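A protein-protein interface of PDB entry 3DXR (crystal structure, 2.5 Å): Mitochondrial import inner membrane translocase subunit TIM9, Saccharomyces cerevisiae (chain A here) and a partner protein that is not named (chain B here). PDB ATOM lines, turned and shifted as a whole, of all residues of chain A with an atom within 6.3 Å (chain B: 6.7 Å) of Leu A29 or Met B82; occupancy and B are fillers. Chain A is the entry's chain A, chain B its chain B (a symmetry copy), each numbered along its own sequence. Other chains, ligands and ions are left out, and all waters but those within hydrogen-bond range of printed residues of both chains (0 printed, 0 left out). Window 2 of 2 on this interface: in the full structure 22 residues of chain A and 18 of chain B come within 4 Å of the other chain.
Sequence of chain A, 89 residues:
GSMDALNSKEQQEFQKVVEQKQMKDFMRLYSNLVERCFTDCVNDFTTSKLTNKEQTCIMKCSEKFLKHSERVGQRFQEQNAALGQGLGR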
ATOM      1  N   LYS A  24      14.367 -36.649  27.816  1.00  0.00           N
ATOM      2  CA  LYS A  24      15.293 -37.406  26.990  1.00  0.00           C
ATOM      3  C   LYS A  24      15.296 -36.834  25.577  1.00  0.00           C
ATOM      4  O   LYS A  24      16.339 -36.756  24.929  1.00  0.00           O
ATOM      5  CB  LYS A  24      14.878 -38.880  26.952  1.00  0.00           C
ATOM      6  N   ASP A  25      14.117 -36.431  25.116  1.00  0.00           N
ATOM      7  CA  ASP A  25      13.956 -35.856  23.787  1.00  0.00           C
ATOM      8  C   ASP A  25      14.761 -34.567  23.658  1.00  0.00           C
ATOM      9  O   ASP A  25      15.441 -34.353  22.651  1.00  0.00           O
ATOM     10  CB  ASP A  25      12.478 -35.564  23.512  1.00  0.00           C
ATOM     11  N   PHE A  26      14.682 -33.713  24.675  1.00  0.00           N
ATOM     12  CA  PHE A  26      15.406 -32.448  24.657  1.00  0.00           C
ATOM     13  C   PHE A  26      16.909 -32.705  24.665  1.00  0.00           C
ATOM     14  O   PHE A  26      17.674 -32.034  23.972  1.00  0.00           O
ATOM     15  CB  PHE A  26      15.042 -31.592  25.870  1.00  0.00           C
ATOM     16  CG  PHE A  26      15.558 -30.180  25.788  1.00  0.00           C
ATOM     17  CD1 PHE A  26      14.894 -29.229  25.020  1.00  0.00           C
ATOM     18  CD2 PHE A  26      16.738 -29.815  26.430  1.00  0.00           C
ATOM     19  CE1 PHE A  26      15.391 -27.933  24.897  1.00  0.00           C
ATOM     20  CE2 PHE A  26      17.247 -28.520  26.313  1.00  0.00           C
ATOM     21  CZ  PHE A  26      16.575 -27.579  25.542  1.00  0.00           C
ATOM     22  N   MET A  27      17.330 -33.672  25.468  1.00  0.00           N
ATOM     23  CA  MET A  27      18.736 -34.010  25.550  1.00  0.00           C
ATOM     24  C   MET A  27      19.172 -34.534  24.194  1.00  0.00           C
ATOM     25  O   MET A  27      20.354 -34.506  23.854  1.00  0.00           O
ATOM     26  CB  MET A  27      18.961 -35.066  26.629  1.00  0.00           C
ATOM     27  CG  MET A  27      18.655 -34.579  28.034  1.00  0.00           C
ATOM     28  SD  MET A  27      19.094 -35.797  29.293  1.00  0.00           S
ATOM     29  CE  MET A  27      17.484 -36.194  29.956  1.00  0.00           C
ATOM     30  N   ARG A  28      18.200 -35.005  23.421  1.00  0.00           N
ATOM     31  CA  ARG A  28      18.459 -35.533  22.089  1.00  0.00           C
ATOM     32  C   ARG A  28      18.854 -34.413  21.128  1.00  0.00           C
ATOM     33  O   ARG A  28      19.983 -34.381  20.641  1.00  0.00           O
ATOM     34  CB  ARG A  28      17.218 -36.261  21.559  1.00  0.00           C
ATOM     35  N   LEU A  29      17.931 -33.493  20.864  1.00  0.00           N
ATOM     36  CA  LEU A  29      18.215 -32.384  19.964  1.00  0.00           C
ATOM     37  C   LEU A  29      19.572 -31.773  20.272  1.00  0.00           C
ATOM     38  O   LEU A  29      20.470 -31.767  19.426  1.00  0.00           O
ATOM     39  CB  LEU A  29      17.139 -31.300  20.077  1.00  0.00           C
ATOM     40  CG  LEU A  29      17.462 -29.998  19.327  1.00  0.00           C
ATOM     41  CD1 LEU A  29      17.705 -30.293  17.848  1.00  0.00           C
ATOM     42  CD2 LEU A  29      16.325 -28.999  19.497  1.00  0.00           C
ATOM     43  N   TYR A  30      19.708 -31.260  21.489  1.00  0.00           N
ATOM     44  CA  TYR A  30      20.943 -30.631  21.942  1.00  0.00           C
ATOM     45  C   TYR A  30      22.161 -31.417  21.467  1.00  0.00           C
ATOM     46  O   TYR A  30      23.057 -30.869  20.836  1.00  0.00           O
ATOM     47  CB  TYR A  30      20.946 -30.542  23.473  1.00  0.00           C
ATOM     48  CG  TYR A  30      22.284 -30.163  24.070  1.00  0.00           C
ATOM     49  CD1 TYR A  30      22.791 -28.867  23.938  1.00  0.00           C
ATOM     50  CD2 TYR A  30      23.060 -31.111  24.747  1.00  0.00           C
ATOM     51  CE1 TYR A  30      24.038 -28.524  24.466  1.00  0.00           C
ATOM     52  CE2 TYR A  30      24.308 -30.779  25.276  1.00  0.00           C
ATOM     53  CZ  TYR A  30      24.790 -29.484  25.131  1.00  0.00           C
ATOM     54  OH  TYR A  30      26.026 -29.155  25.646  1.00  0.00           O
ATOM     55  N   SER A  31      22.166 -32.707  21.777  1.00  0.00           N
ATOM     56  CA  SER A  31      23.252 -33.605  21.418  1.00  0.00           C
ATOM     57  C   SER A  31      23.452 -33.693  19.899  1.00  0.00           C
ATOM     58  O   SER A  31      24.563 -33.510  19.392  1.00  0.00           O
ATOM     59  CB  SER A  31      22.963 -34.994  21.994  1.00  0.00           C
ATOM     60  OG  SER A  31      24.161 -35.693  22.280  1.00  0.00           O
ATOM     61  N   ASN A  32      22.367 -33.974  19.184  1.00  0.00           N
ATOM     62  CA  ASN A  32      22.397 -34.092  17.731  1.00  0.00           C
ATOM     63  C   ASN A  32      22.823 -32.779  17.104  1.00  0.00           C
ATOM     64  O   ASN A  32      23.489 -32.761  16.072  1.00  0.00           O
ATOM     65  CB  ASN A  32      21.016 -34.469  17.190  1.00  0.00           C
ATOM     66  CG  ASN A  32      20.519 -35.788  17.731  1.00  0.00           C
ATOM     67  OD1 ASN A  32      21.268 -36.764  17.804  1.00  0.00           O
ATOM     68  ND2 ASN A  32      19.246 -35.832  18.109  1.00  0.00           N
ATOM     69  N   LEU A  33      22.419 -31.680  17.726  1.00  0.00           N
ATOM     70  CA  LEU A  33      22.770 -30.367  17.226  1.00  0.00           C
ATOM     71  C   LEU A  33      24.262 -30.150  17.395  1.00  0.00           C
ATOM     72  O   LEU A  33      24.948 -29.703  16.481  1.00  0.00           O
ATOM     73  CB  LEU A  33      21.996 -29.289  17.981  1.00  0.00           C
ATOM     74  CG  LEU A  33      22.310 -27.847  17.569  1.00  0.00           C
ATOM     75  CD1 LEU A  33      22.150 -27.685  16.064  1.00  0.00           C
ATOM     76  CD2 LEU A  33      21.395 -26.893  18.320  1.00  0.00           C
ATOM     77  N   VAL A  34      24.761 -30.468  18.577  1.00  0.00           N
ATOM     78  CA  VAL A  34      26.173 -30.305  18.861  1.00  0.00           C
ATOM     79  C   VAL A  34      26.979 -31.096  17.829  1.00  0.00           C
ATOM     80  O   VAL A  34      27.903 -30.567  17.210  1.00  0.00           O
ATOM     81  CB  VAL A  34      26.513 -30.812  20.289  1.00  0.00           C
ATOM     82  CG1 VAL A  34      27.996 -30.662  20.560  1.00  0.00           C
ATOM     83  CG2 VAL A  34      25.717 -30.028  21.324  1.00  0.00           C
ATOM     84  N   SER A  62      23.583 -23.750  13.937  1.00  0.00           N
ATOM     85  CA  SER A  62      22.628 -23.828  15.044  1.00  0.00           C
ATOM     86  C   SER A  62      21.253 -23.348  14.605  1.00  0.00           C
ATOM     87  O   SER A  62      20.237 -24.014  14.813  1.00  0.00           O
ATOM     88  CB  SER A  62      23.090 -22.946  16.211  1.00  0.00           C
ATOM     89  OG  SER A  62      24.291 -23.424  16.786  1.00  0.00           O
ATOM     90  N   PHE A  65      19.653 -25.481  11.676  1.00  0.00           N
ATOM     91  CA  PHE A  65      19.190 -26.756  12.187  1.00  0.00           C
ATOM     92  C   PHE A  65      17.950 -26.635  13.045  1.00  0.00           C
ATOM     93  O   PHE A  65      17.006 -27.398  12.872  1.00  0.00           O
ATOM     94  CB  PHE A  65      20.295 -27.467  12.973  1.00  0.00           C
ATOM     95  CG  PHE A  65      19.986 -28.912  13.249  1.00  0.00           C
ATOM     96  CD1 PHE A  65      19.766 -29.795  12.196  1.00  0.00           C
ATOM     97  CD2 PHE A  65      19.852 -29.377  14.552  1.00  0.00           C
ATOM     98  CE1 PHE A  65      19.410 -31.114  12.437  1.00  0.00           C
ATOM     99  CE2 PHE A  65      19.496 -30.694  14.803  1.00  0.00           C
ATOM    100  CZ  PHE A  65      19.275 -31.564  13.742  1.00  0.00           C
ATOM    101  N   LEU A  66      17.945 -25.679  13.971  1.00  0.00           N
ATOM    102  CA  LEU A  66      16.779 -25.471  14.836  1.00  0.00           C
ATOM    103  C   LEU A  66      15.570 -25.096  13.992  1.00  0.00           C
ATOM    104  O   LEU A  66      14.460 -25.584  14.225  1.00  0.00           O
ATOM    105  CB  LEU A  66      17.052 -24.375  15.872  1.00  0.00           C
ATOM    106  CG  LEU A  66      17.990 -24.763  17.025  1.00  0.00           C
ATOM    107  CD1 LEU A  66      18.110 -23.606  18.015  1.00  0.00           C
ATOM    108  CD2 LEU A  66      17.449 -26.000  17.726  1.00  0.00           C
ATOM    109  N   SER A  69      14.512 -28.141  12.101  1.00  0.00           N
ATOM    110  CA  SER A  69      13.935 -29.026  13.091  1.00  0.00           C
ATOM    111  C   SER A  69      12.549 -28.550  13.528  1.00  0.00           C
ATOM    112  O   SER A  69      11.690 -29.355  13.913  1.00  0.00           O
ATOM    113  CB  SER A  69      14.879 -29.113  14.294  1.00  0.00           C
ATOM    114  OG  SER A  69      14.528 -30.197  15.133  1.00  0.00           O
ATOM    115  N   GLN B  77      29.031 -23.349  23.235  1.00  0.00           N
ATOM    116  CA  GLN B  77      28.673 -22.455  22.141  1.00  0.00           C
ATOM    117  C   GLN B  77      27.234 -22.744  21.698  1.00  0.00           C
ATOM    118  O   GLN B  77      26.391 -21.848  21.677  1.00  0.00           O
ATOM    119  CB  GLN B  77      29.623 -22.661  20.961  1.00  0.00           C
ATOM    120  CG  GLN B  77      29.497 -21.601  19.890  1.00  0.00           C
ATOM    121  CD  GLN B  77      30.168 -20.304  20.287  1.00  0.00           C
ATOM    122  OE1 GLN B  77      30.441 -20.067  21.464  1.00  0.00           O
ATOM    123  NE2 GLN B  77      30.427 -19.448  19.309  1.00  0.00           N
ATOM    124  N   VAL B  78      26.964 -23.998  21.346  1.00  0.00           N
ATOM    125  CA  VAL B  78      25.633 -24.412  20.909  1.00  0.00           C
ATOM    126  C   VAL B  78      24.622 -24.248  22.044  1.00  0.00           C
ATOM    127  O   VAL B  78      23.435 -24.044  21.809  1.00  0.00           O
ATOM    128  CB  VAL B  78      25.649 -25.887  20.437  1.00  0.00           C
ATOM    129  CG1 VAL B  78      24.237 -26.380  20.158  1.00  0.00           C
ATOM    130  CG2 VAL B  78      26.504 -26.010  19.192  1.00  0.00           C
ATOM    131  N   GLY B  79      25.101 -24.343  23.277  1.00  0.00           N
ATOM    132  CA  GLY B  79      24.220 -24.181  24.420  1.00  0.00           C
ATOM    133  C   GLY B  79      23.775 -22.731  24.542  1.00  0.00           C
ATOM    134  O   GLY B  79      22.623 -22.447  24.863  1.00  0.00           O
ATOM    135  N   GLU B  80      24.694 -21.808  24.282  1.00  0.00           N
ATOM    136  CA  GLU B  80      24.387 -20.385  24.353  1.00  0.00           C
ATOM    137  C   GLU B  80      23.529 -19.949  23.165  1.00  0.00           C
ATOM    138  O   GLU B  80      22.805 -18.960  23.255  1.00  0.00           O
ATOM    139  CB  GLU B  80      25.682 -19.557  24.399  1.00  0.00           C
ATOM    140  CG  GLU B  80      26.571 -19.856  25.607  1.00  0.00           C
ATOM    141  CD  GLU B  80      27.795 -18.953  25.696  1.00  0.00           C
ATOM    142  OE1 GLU B  80      28.552 -18.869  24.706  1.00  0.00           O
ATOM    143  OE2 GLU B  80      28.004 -18.331  26.761  1.00  0.00           O
ATOM    144  N   ASN B  81      23.608 -20.685  22.057  1.00  0.00           N
ATOM    145  CA  ASN B  81      22.826 -20.361  20.863  1.00  0.00           C
ATOM    146  C   ASN B  81      21.356 -20.716  21.068  1.00  0.00           C
ATOM    147  O   ASN B  81      20.466 -20.034  20.555  1.00  0.00           O
ATOM    148  CB  ASN B  81      23.359 -21.108  19.633  1.00  0.00           C
ATOM    149  CG  ASN B  81      24.758 -20.664  19.231  1.00  0.00           C
ATOM    150  OD1 ASN B  81      25.027 -19.470  19.083  1.00  0.00           O
ATOM    151  ND2 ASN B  81      25.654 -21.629  19.041  1.00  0.00           N
ATOM    152  N   MET B  82      21.106 -21.791  21.810  1.00  0.00           N
ATOM    153  CA  MET B  82      19.743 -22.217  22.094  1.00  0.00           C
ATOM    154  C   MET B  82      19.132 -21.297  23.151  1.00  0.00           C
ATOM    155  O   MET B  82      17.922 -21.065  23.170  1.00  0.00           O
ATOM    156  CB  MET B  82      19.728 -23.662  22.594  1.00  0.00           C
ATOM    157  CG  MET B  82      20.239 -24.675  21.584  1.00  0.00           C
ATOM    158  SD  MET B  82      19.943 -26.384  22.094  1.00  0.00           S
ATOM    159  CE  MET B  82      18.218 -26.524  21.734  1.00  0.00           C
ATOM    160  N   GLN B  83      19.984 -20.776  24.030  1.00  0.00           N
ATOM    161  CA  GLN B  83      19.544 -19.873  25.085  1.00  0.00           C
ATOM    162  C   GLN B  83      19.141 -18.523  24.499  1.00  0.00           C
ATOM    163  O   GLN B  83      18.279 -17.834  25.042  1.00  0.00           O
ATOM    164  CB  GLN B  83      20.664 -19.671  26.114  1.00  0.00           C
ATOM    165  N   LYS B  84      19.769 -18.148  23.391  1.00  0.00           N
ATOM    166  CA  LYS B  84      19.457 -16.882  22.747  1.00  0.00           C
ATOM    167  C   LYS B  84      18.067 -16.935  22.140  1.00  0.00           C
ATOM    168  O   LYS B  84      17.252 -16.044  22.366  1.00  0.00           O
ATOM    169  CB  LYS B  84      20.484 -16.566  21.664  1.00  0.00           C
ATOM    170  CG  LYS B  84      20.248 -15.239  20.971  1.00  0.00           C
ATOM    171  CD  LYS B  84      21.370 -14.927  20.001  1.00  0.00           C
ATOM    172  CE  LYS B  84      21.152 -13.588  19.329  1.00  0.00           C
ATOM    173  NZ  LYS B  84      22.241 -13.295  18.359  1.00  0.00           N
ATOM    174  N   MET B  85      17.798 -17.980  21.367  1.00  0.00           N
ATOM    175  CA  MET B  85      16.496 -18.142  20.739  1.00  0.00           C
ATOM    176  C   MET B  85      15.769 -19.338  21.340  1.00  0.00           C
ATOM    177  O   MET B  85      14.621 -19.576  20.911  1.00  0.00           O
ATOM    178  CB  MET B  85      16.655 -18.341  19.226  1.00  0.00           C
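The side-chain hydroxyl (OG) of Ser A62 sits at hydrogen-bond distance from the side-chain amide nitrogen (ND2) of Asn B81, at 3.2 Å.
O of Gln B77 is in hydrogen-bond range of ND2 of Asn B81, at 2.7 Å.
Leu A29 touches Met B82 (CD2 to CE, 3.8 Å). Leu A33 touches Val B78 (CD2 to CG1, 3.4 Å).
Lys A24 touches none of the printed residues of chain B. Of chain B, only Met B82 (3.8 Å) comes within 4 Å of Leu A29. Tyr A30 touches none of the printed residues of chain B. Printed residues of chain B within 4 Å of Leu A33: Val B78 (3.4 Å). Of the printed residues of chain B, Ser A62 touches Asn B81. Of the printed residues of chain A, Val B78 touches Leu A33. Of the printed residues of chain A, Asn B81 touches Ser A62. Met B82 touches just one residue of chain A: Leu A29. The nearest residue of chain B that does not touch Leu A29 is Val B78 (6.6 Å). The nearest residue of chain A that does not touch Met B82 is Leu A33 (4.1 Å). The nearest printed residue of chain B that does not touch Ser A62 is Val B78 (4.2 Å).
Hydrophobic or aromatic side chains of chain A within 4 Å of the printed part of chain B: Leu A29 and Leu A33. Hydrophobic or aromatic side chains of chain B that line the printed part of chain A: Val B78 and Met B82. Among the printed residues, no Asp or Glu carboxylate lies within 4 Å of a Lys or Arg side-chain nitrogen of the other chain.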
